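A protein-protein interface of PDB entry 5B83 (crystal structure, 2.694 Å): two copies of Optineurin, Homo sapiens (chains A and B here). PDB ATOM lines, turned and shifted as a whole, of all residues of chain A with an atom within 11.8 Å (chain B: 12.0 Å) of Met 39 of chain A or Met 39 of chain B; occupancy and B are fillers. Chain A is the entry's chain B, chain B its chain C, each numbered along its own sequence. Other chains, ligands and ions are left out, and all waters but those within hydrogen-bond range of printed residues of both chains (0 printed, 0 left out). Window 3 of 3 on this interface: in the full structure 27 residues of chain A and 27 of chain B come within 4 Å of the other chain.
Among the printed residues, pairs that only touch across the chains: Thr 42 of chain A with Ile 43 of chain B (3.2 Å), Met 39 of chain A with Met 39 of chain B (3.3 Å), Ile 43 of chain A with Thr 42 of chain B (3.3 Å), Ile 43 of chain A with Ile 43 of chain B (3.3 Å), Thr 42 of chain A with Gln 46 of chain B (3.6 Å) and Met 39 of chain A with Ile 43 of chain B (3.6 Å).
N of Met 39 of chain B is in hydrogen-bond range of OD1 of Asp 37 of chain B (3.1 Å). The backbone carbonyl oxygen of Met 39 of chain B lies within hydrogen-bond range of the side-chain hydroxyl of Thr 42 of chain B (3.4 Å). O of Met 39 of chain A lies within hydrogen-bond range of OG1 of Thr 42 of chain A (3.1 Å). O of Ile 43 of chain A sits close to OE1 of Gln 46 of chain A. OG1 of Thr 42 of chain A sits at hydrogen-bond distance from O of Glu 38 of chain A (2.9 Å).
Of the 14 printed residues of chain A, 4 touch a printed residue of chain B. Of the 12 printed residues of chain B, 4 touch a printed residue of chain A. Hydrophobic or aromatic side chains of chain B that line the printed part of chain A: Met 39 and Ile 43. Among the printed residues, 7 pairs touch across the chains. Among the printed residues, no Asp or Glu carboxylate lies within 4 Å of a Lys or Arg side-chain nitrogen of the other chain.
OE1 of Gln 46 of chain A lies close to OE1 of Gln 46 of chain B (2.9 Å).
Met 39 of chain A touches its own counterpart, Met 39 of chain B. Met 39 of chain A touches Ile 43 of chain B, but with the chains exchanged Ile 43 of chain A does not touch Met 39 of chain B (4.8 Å). Thr 42 of chain A touches Ile 43 of chain B, and with the chains exchanged Ile 43 of chain A touches Thr 42 of chain B. Gln 46 of chain A touches its own counterpart, Gln 46 of chain B.
Of the printed residues of chain B, Met 39 of chain A touches Met 39 and Ile 43. Of chain A, only Met 39 (3.3 Å) comes within 4 Å of Met 39 of chain B. Asp 37 of chain A touches none of the printed residues of chain B. No residue of chain B comes within 4 Å of Glu 38 of chain A. No residue of chain B comes within 4 Å of Lys 40 of chain A. Thr 42 of chain A touches just these residues of chain B: Ile 43 (3.2 Å) and Gln 46 (3.6 Å). Of chain B, only Thr 42 (3.3 Å) and Ile 43 (3.3 Å) come within 4 Å of Ile 43 of chain A. No residue of chain A comes within 4 Å of Glu 38 of chain B. Lys 40 of chain B touches none of the printed residues of chain A. Gln 41 of chain B touches none of the printed residues of chain A. Of the printed residues of chain B, Gln 46 of chain A touches Gln 46 (2.9 Å). Of the printed residues of chain A, Gln 46 of chain B touches Thr 42 (3.6 Å) and Gln 46 (2.9 Å). Met 36 of chain A touches none of the printed residues of chain B. The nearest printed residue of chain A that does not touch Gln 46 of chain B is Ile 43 of chain A (4.3 Å).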
ATOM      1  N   GLN A  35       1.099  21.344  -3.701  1.00  0.00           N
ATOM      2  CA  GLN A  35       0.731  20.220  -2.835  1.00  0.00           C
ATOM      3  C   GLN A  35      -0.093  19.147  -3.606  1.00  0.00           C
ATOM      4  O   GLN A  35      -1.139  18.673  -3.145  1.00  0.00           O
ATOM      5  CB  GLN A  35      -0.021  20.747  -1.593  1.00  0.00           C
ATOM      6  CG  GLN A  35       0.907  21.437  -0.535  1.00  0.00           C
ATOM      7  CD  GLN A  35       0.167  22.209   0.600  1.00  0.00           C
ATOM      8  OE1 GLN A  35      -1.004  22.576   0.465  1.00  0.00           O
ATOM      9  NE2 GLN A  35       0.872  22.461   1.713  1.00  0.00           N
ATOM     10  N   MET A  36       0.418  18.766  -4.782  1.00  0.00           N
ATOM     11  CA  MET A  36      -0.222  17.780  -5.650  1.00  0.00           C
ATOM     12  C   MET A  36       0.209  16.366  -5.291  1.00  0.00           C
ATOM     13  O   MET A  36       1.393  16.096  -5.069  1.00  0.00           O
ATOM     14  CB  MET A  36       0.122  18.014  -7.121  1.00  0.00           C
ATOM     15  CG  MET A  36       0.033  19.428  -7.585  1.00  0.00           C
ATOM     16  SD  MET A  36      -1.623  20.073  -7.414  1.00  0.00           S
ATOM     17  CE  MET A  36      -1.216  21.780  -7.029  1.00  0.00           C
ATOM     18  N   ASP A  37      -0.757  15.452  -5.295  1.00  0.00           N
ATOM     19  CA  ASP A  37      -0.474  14.067  -4.948  1.00  0.00           C
ATOM     20  C   ASP A  37      -0.894  13.116  -6.063  1.00  0.00           C
ATOM     21  O   ASP A  37      -1.726  12.231  -5.848  1.00  0.00           O
ATOM     22  CB  ASP A  37      -1.167  13.701  -3.628  1.00  0.00           C
ATOM     23  CG  ASP A  37      -0.580  14.439  -2.429  1.00  0.00           C
ATOM     24  OD1 ASP A  37       0.659  14.561  -2.354  1.00  0.00           O
ATOM     25  OD2 ASP A  37      -1.355  14.901  -1.563  1.00  0.00           O
ATOM     26  N   GLU A  38      -0.326  13.290  -7.259  1.00  0.00           N
ATOM     27  CA  GLU A  38      -0.397  12.235  -8.261  1.00  0.00           C
ATOM     28  C   GLU A  38       0.395  11.011  -7.838  1.00  0.00           C
ATOM     29  O   GLU A  38       0.373  10.002  -8.553  1.00  0.00           O
ATOM     30  CB  GLU A  38       0.131  12.704  -9.613  1.00  0.00           C
ATOM     31  CG  GLU A  38       1.212  13.748  -9.539  1.00  0.00           C
ATOM     32  CD  GLU A  38       0.673  15.119  -9.871  1.00  0.00           C
ATOM     33  OE1 GLU A  38       1.187  16.124  -9.330  1.00  0.00           O
ATOM     34  OE2 GLU A  38      -0.278  15.184 -10.677  1.00  0.00           O
ATOM     35  N   MET A  39       1.117  11.090  -6.716  1.00  0.00           N
ATOM     36  CA  MET A  39       1.622   9.914  -6.029  1.00  0.00           C
ATOM     37  C   MET A  39       0.533   8.862  -5.881  1.00  0.00           C
ATOM     38  O   MET A  39       0.794   7.670  -6.043  1.00  0.00           O
ATOM     39  CB  MET A  39       2.165  10.315  -4.669  1.00  0.00           C
ATOM     40  CG  MET A  39       1.198  11.086  -3.752  1.00  0.00           C
ATOM     41  SD  MET A  39       0.409  10.046  -2.501  1.00  0.00           S
ATOM     42  CE  MET A  39       0.153  11.207  -1.170  1.00  0.00           C
ATOM     43  N   LYS A  40      -0.684   9.295  -5.556  1.00  0.00           N
ATOM     44  CA  LYS A  40      -1.814   8.380  -5.510  1.00  0.00           C
ATOM     45  C   LYS A  40      -1.973   7.656  -6.835  1.00  0.00           C
ATOM     46  O   LYS A  40      -2.123   6.432  -6.878  1.00  0.00           O
ATOM     47  CB  LYS A  40      -3.094   9.148  -5.169  1.00  0.00           C
ATOM     48  CG  LYS A  40      -3.030   9.876  -3.839  1.00  0.00           C
ATOM     49  CD  LYS A  40      -2.959   8.887  -2.683  1.00  0.00           C
ATOM     50  CE  LYS A  40      -3.976   9.225  -1.600  1.00  0.00           C
ATOM     51  NZ  LYS A  40      -4.091   8.133  -0.601  1.00  0.00           N
ATOM     52  N   GLN A  41      -1.926   8.409  -7.931  1.00  0.00           N
ATOM     53  CA  GLN A  41      -2.042   7.820  -9.256  1.00  0.00           C
ATOM     54  C   GLN A  41      -0.877   6.890  -9.557  1.00  0.00           C
ATOM     55  O   GLN A  41      -1.058   5.838 -10.185  1.00  0.00           O
ATOM     56  CB  GLN A  41      -2.126   8.926 -10.305  1.00  0.00           C
ATOM     57  CG  GLN A  41      -1.501   8.564 -11.639  1.00  0.00           C
ATOM     58  CD  GLN A  41      -2.122   9.320 -12.796  1.00  0.00           C
ATOM     59  OE1 GLN A  41      -2.764  10.355 -12.603  1.00  0.00           O
ATOM     60  NE2 GLN A  41      -1.944   8.797 -14.008  1.00  0.00           N
ATOM     61  N   THR A  42       0.328   7.254  -9.121  1.00  0.00           N
ATOM     62  CA  THR A  42       1.464   6.390  -9.408  1.00  0.00           C
ATOM     63  C   THR A  42       1.561   5.226  -8.424  1.00  0.00           C
ATOM     64  O   THR A  42       2.038   4.154  -8.807  1.00  0.00           O
ATOM     65  CB  THR A  42       2.762   7.203  -9.448  1.00  0.00           C
ATOM     66  OG1 THR A  42       2.723   8.227  -8.448  1.00  0.00           O
ATOM     67  CG2 THR A  42       2.948   7.853 -10.816  1.00  0.00           C
ATOM     68  N   ILE A  43       1.095   5.384  -7.179  1.00  0.00           N
ATOM     69  CA  ILE A  43       0.922   4.214  -6.313  1.00  0.00           C
ATOM     70  C   ILE A  43      -0.092   3.253  -6.925  1.00  0.00           C
ATOM     71  O   ILE A  43       0.149   2.046  -7.029  1.00  0.00           O
ATOM     72  CB  ILE A  43       0.493   4.620  -4.890  1.00  0.00           C
ATOM     73  CG1 ILE A  43       1.595   5.362  -4.143  1.00  0.00           C
ATOM     74  CG2 ILE A  43       0.145   3.388  -4.084  1.00  0.00           C
ATOM     75  CD1 ILE A  43       1.168   5.842  -2.751  1.00  0.00           C
ATOM     76  N   ALA A  44      -1.255   3.780  -7.323  1.00  0.00           N
ATOM     77  CA  ALA A  44      -2.291   2.945  -7.919  1.00  0.00           C
ATOM     78  C   ALA A  44      -1.799   2.262  -9.190  1.00  0.00           C
ATOM     79  O   ALA A  44      -2.231   1.147  -9.498  1.00  0.00           O
ATOM     80  CB  ALA A  44      -3.540   3.781  -8.201  1.00  0.00           C
ATOM     81  N   LYS A  45      -0.895   2.908  -9.932  1.00  0.00           N
ATOM     82  CA  LYS A  45      -0.275   2.276 -11.092  1.00  0.00           C
ATOM     83  C   LYS A  45       0.715   1.192 -10.684  1.00  0.00           C
ATOM     84  O   LYS A  45       0.944   0.253 -11.451  1.00  0.00           O
ATOM     85  CB  LYS A  45       0.406   3.350 -11.941  1.00  0.00           C
ATOM     86  CG  LYS A  45       1.468   2.859 -12.922  1.00  0.00           C
ATOM     87  CD  LYS A  45       0.859   2.285 -14.193  1.00  0.00           C
ATOM     88  CE  LYS A  45       1.916   2.104 -15.288  1.00  0.00           C
ATOM     89  NZ  LYS A  45       2.819   0.954 -15.029  1.00  0.00           N
ATOM     90  N   GLN A  46       1.283   1.288  -9.484  1.00  0.00           N
ATOM     91  CA  GLN A  46       2.127   0.222  -8.962  1.00  0.00           C
ATOM     92  C   GLN A  46       1.305  -0.945  -8.438  1.00  0.00           C
ATOM     93  O   GLN A  46       1.703  -2.104  -8.605  1.00  0.00           O
ATOM     94  CB  GLN A  46       3.011   0.767  -7.846  1.00  0.00           C
ATOM     95  CG  GLN A  46       3.058  -0.095  -6.574  1.00  0.00           C
ATOM     96  CD  GLN A  46       3.212   0.730  -5.300  1.00  0.00           C
ATOM     97  OE1 GLN A  46       2.854   1.903  -5.270  1.00  0.00           O
ATOM     98  NE2 GLN A  46       3.758   0.120  -4.248  1.00  0.00           N
ATOM     99  N   GLU A  47       0.174  -0.657  -7.778  1.00  0.00           N
ATOM    100  CA  GLU A  47      -0.631  -1.725  -7.194  1.00  0.00           C
ATOM    101  C   GLU A  47      -1.080  -2.711  -8.263  1.00  0.00           C
ATOM    102  O   GLU A  47      -0.992  -3.931  -8.073  1.00  0.00           O
ATOM    103  CB  GLU A  47      -1.833  -1.134  -6.452  1.00  0.00           C
ATOM    104  CG  GLU A  47      -1.465  -0.250  -5.250  1.00  0.00           C
ATOM    105  CD  GLU A  47      -2.651   0.055  -4.340  1.00  0.00           C
ATOM    106  OE1 GLU A  47      -3.475  -0.856  -4.110  1.00  0.00           O
ATOM    107  OE2 GLU A  47      -2.763   1.207  -3.859  1.00  0.00           O
ATOM    108  N   GLU A  48      -1.542  -2.195  -9.407  1.00  0.00           N
ATOM    109  CA  GLU A  48      -1.830  -3.043 -10.555  1.00  0.00           C
ATOM    110  C   GLU A  48      -0.605  -3.851 -10.942  1.00  0.00           C
ATOM    111  O   GLU A  48      -0.645  -5.085 -11.001  1.00  0.00           O
ATOM    112  CB  GLU A  48      -2.293  -2.195 -11.738  1.00  0.00           C
ATOM    113  CG  GLU A  48      -3.768  -1.871 -11.729  1.00  0.00           C
ATOM    114  CD  GLU A  48      -4.087  -0.662 -12.587  1.00  0.00           C
ATOM    115  OE1 GLU A  48      -3.543  -0.600 -13.719  1.00  0.00           O
ATOM    116  OE2 GLU A  48      -4.859   0.224 -12.115  1.00  0.00           O
ATOM    117  N   ASP B  37       4.585  15.381   4.211  1.00  0.00           N
ATOM    118  CA  ASP B  37       4.324  14.561   3.024  1.00  0.00           C
ATOM    119  C   ASP B  37       5.266  13.346   2.929  1.00  0.00           C
ATOM    120  O   ASP B  37       6.436  13.477   2.553  1.00  0.00           O
ATOM    121  CB  ASP B  37       4.431  15.430   1.757  1.00  0.00           C
ATOM    122  CG  ASP B  37       4.268  14.627   0.456  1.00  0.00           C
ATOM    123  OD1 ASP B  37       3.818  13.455   0.492  1.00  0.00           O
ATOM    124  OD2 ASP B  37       4.582  15.188  -0.617  1.00  0.00           O
ATOM    125  N   GLU B  38       4.751  12.161   3.247  1.00  0.00           N
ATOM    126  CA  GLU B  38       5.538  10.935   3.193  1.00  0.00           C
ATOM    127  C   GLU B  38       4.943   9.934   2.209  1.00  0.00           C
ATOM    128  O   GLU B  38       4.895   8.726   2.461  1.00  0.00           O
ATOM    129  CB  GLU B  38       5.671  10.309   4.576  1.00  0.00           C
ATOM    130  CG  GLU B  38       6.836   9.340   4.685  1.00  0.00           C
ATOM    131  CD  GLU B  38       6.737   8.470   5.907  1.00  0.00           C
ATOM    132  OE1 GLU B  38       5.912   8.791   6.789  1.00  0.00           O
ATOM    133  OE2 GLU B  38       7.478   7.467   5.981  1.00  0.00           O
ATOM    134  N   MET B  39       4.465  10.435   1.068  1.00  0.00           N
ATOM    135  CA  MET B  39       4.092   9.547  -0.033  1.00  0.00           C
ATOM    136  C   MET B  39       5.284   8.725  -0.479  1.00  0.00           C
ATOM    137  O   MET B  39       5.164   7.521  -0.710  1.00  0.00           O
ATOM    138  CB  MET B  39       3.551  10.355  -1.216  1.00  0.00           C
ATOM    139  CG  MET B  39       4.503  10.479  -2.416  1.00  0.00           C
ATOM    140  SD  MET B  39       4.804  12.177  -2.948  1.00  0.00           S
ATOM    141  CE  MET B  39       5.166  11.958  -4.691  1.00  0.00           C
ATOM    142  N   LYS B  40       6.457   9.361  -0.556  1.00  0.00           N
ATOM    143  CA  LYS B  40       7.691   8.765  -1.049  1.00  0.00           C
ATOM    144  C   LYS B  40       8.080   7.532  -0.259  1.00  0.00           C
ATOM    145  O   LYS B  40       8.967   6.784  -0.691  1.00  0.00           O
ATOM    146  CB  LYS B  40       8.785   9.837  -1.001  1.00  0.00           C
ATOM    147  CG  LYS B  40       8.317  11.108  -0.276  1.00  0.00           C
ATOM    148  CD  LYS B  40       9.238  12.289  -0.540  1.00  0.00           C
ATOM    149  CE  LYS B  40       8.956  13.448   0.401  1.00  0.00           C
ATOM    150  NZ  LYS B  40       9.960  14.521   0.192  1.00  0.00           N
ATOM    151  N   GLN B  41       7.424   7.312   0.885  1.00  0.00           N
ATOM    152  CA  GLN B  41       7.584   6.089   1.658  1.00  0.00           C
ATOM    153  C   GLN B  41       7.402   4.840   0.808  1.00  0.00           C
ATOM    154  O   GLN B  41       8.068   3.827   1.046  1.00  0.00           O
ATOM    155  CB  GLN B  41       6.577   6.098   2.811  1.00  0.00           C
ATOM    156  CG  GLN B  41       6.735   4.957   3.780  1.00  0.00           C
ATOM    157  CD  GLN B  41       8.120   4.916   4.389  1.00  0.00           C
ATOM    158  OE1 GLN B  41       8.753   5.953   4.600  1.00  0.00           O
ATOM    159  NE2 GLN B  41       8.603   3.714   4.667  1.00  0.00           N
ATOM    160  N   THR B  42       6.521   4.888  -0.192  1.00  0.00           N
ATOM    161  CA  THR B  42       6.169   3.711  -0.975  1.00  0.00           C
ATOM    162  C   THR B  42       6.612   3.792  -2.429  1.00  0.00           C
ATOM    163  O   THR B  42       7.246   2.853  -2.912  1.00  0.00           O
ATOM    164  CB  THR B  42       4.653   3.473  -0.907  1.00  0.00           C
ATOM    165  OG1 THR B  42       3.968   4.488  -1.653  1.00  0.00           O
ATOM    166  CG2 THR B  42       4.177   3.505   0.541  1.00  0.00           C
ATOM    167  N   ILE B  43       6.296   4.888  -3.135  1.00  0.00           N
ATOM    168  CA  ILE B  43       6.577   5.025  -4.572  1.00  0.00           C
ATOM    169  C   ILE B  43       7.977   4.535  -4.925  1.00  0.00           C
ATOM    170  O   ILE B  43       8.197   3.991  -6.016  1.00  0.00           O
ATOM    171  CB  ILE B  43       6.363   6.494  -5.021  1.00  0.00           C
ATOM    172  CG1 ILE B  43       4.882   6.865  -5.029  1.00  0.00           C
ATOM    173  CG2 ILE B  43       6.922   6.732  -6.418  1.00  0.00           C
ATOM    174  CD1 ILE B  43       4.152   6.330  -6.235  1.00  0.00           C
ATOM    175  N   ALA B  44       8.940   4.689  -4.010  1.00  0.00           N
ATOM    176  CA  ALA B  44      10.296   4.214  -4.271  1.00  0.00           C
ATOM    177  C   ALA B  44      10.441   2.718  -3.986  1.00  0.00           C
ATOM    178  O   ALA B  44      11.099   2.001  -4.752  1.00  0.00           O
ATOM    179  CB  ALA B  44      11.304   5.019  -3.447  1.00  0.00           C
ATOM    180  N   LYS B  45       9.844   2.228  -2.893  1.00  0.00           N
ATOM    181  CA  LYS B  45       9.920   0.801  -2.583  1.00  0.00           C
ATOM    182  C   LYS B  45       9.186  -0.033  -3.630  1.00  0.00           C
ATOM    183  O   LYS B  45       9.542  -1.197  -3.868  1.00  0.00           O
ATOM    184  CB  LYS B  45       9.345   0.548  -1.188  1.00  0.00           C
ATOM    185  CG  LYS B  45       9.668  -0.817  -0.607  1.00  0.00           C
ATOM    186  CD  LYS B  45       8.671  -1.188   0.476  1.00  0.00           C
ATOM    187  CE  LYS B  45       7.585  -2.106  -0.067  1.00  0.00           C
ATOM    188  NZ  LYS B  45       8.139  -3.441  -0.418  1.00  0.00           N
ATOM    189  N   GLN B  46       8.168   0.557  -4.260  1.00  0.00           N
ATOM    190  CA  GLN B  46       7.433  -0.101  -5.330  1.00  0.00           C
ATOM    191  C   GLN B  46       8.354  -0.529  -6.464  1.00  0.00           C
ATOM    192  O   GLN B  46       8.206  -1.630  -7.004  1.00  0.00           O
ATOM    193  CB  GLN B  46       6.356   0.846  -5.854  1.00  0.00           C
ATOM    194  CG  GLN B  46       6.431   1.136  -7.346  1.00  0.00           C
ATOM    195  CD  GLN B  46       5.756   2.427  -7.727  1.00  0.00           C
ATOM    196  OE1 GLN B  46       4.923   2.944  -6.985  1.00  0.00           O
ATOM    197  NE2 GLN B  46       6.109   2.958  -8.890  1.00  0.00           N
ATOM    198  N   GLU B  47       9.305   0.331  -6.846  1.00  0.00           N
ATOM    199  CA  GLU B  47      10.130   0.044  -8.016  1.00  0.00           C
ATOM    200  C   GLU B  47      11.090  -1.107  -7.754  1.00  0.00           C
ATOM    201  O   GLU B  47      11.437  -1.838  -8.688  1.00  0.00           O
ATOM    202  CB  GLU B  47      10.900   1.296  -8.448  1.00  0.00           C
ATOM    203  CG  GLU B  47      10.027   2.425  -9.007  1.00  0.00           C
ATOM    204  CD  GLU B  47      10.765   3.766  -9.118  1.00  0.00           C
ATOM    205  OE1 GLU B  47      12.019   3.766  -9.124  1.00  0.00           O
ATOM    206  OE2 GLU B  47      10.090   4.823  -9.194  1.00  0.00           O
ATOM    207  N   LEU B  50       9.128  -4.354  -7.993  1.00  0.00           N
ATOM    208  CA  LEU B  50       8.795  -4.539  -9.399  1.00  0.00           C
ATOM    209  C   LEU B  50      10.014  -4.826 -10.279  1.00  0.00           C
ATOM    210  O   LEU B  50       9.833  -5.181 -11.448  1.00  0.00           O
ATOM    211  CB  LEU B  50       8.043  -3.313  -9.913  1.00  0.00           C
ATOM    212  CG  LEU B  50       6.645  -3.099  -9.293  1.00  0.00           C
ATOM    213  CD1 LEU B  50       6.021  -1.801  -9.769  1.00  0.00           C
ATOM    214  CD2 LEU B  50       5.683  -4.243  -9.569  1.00  0.00           C
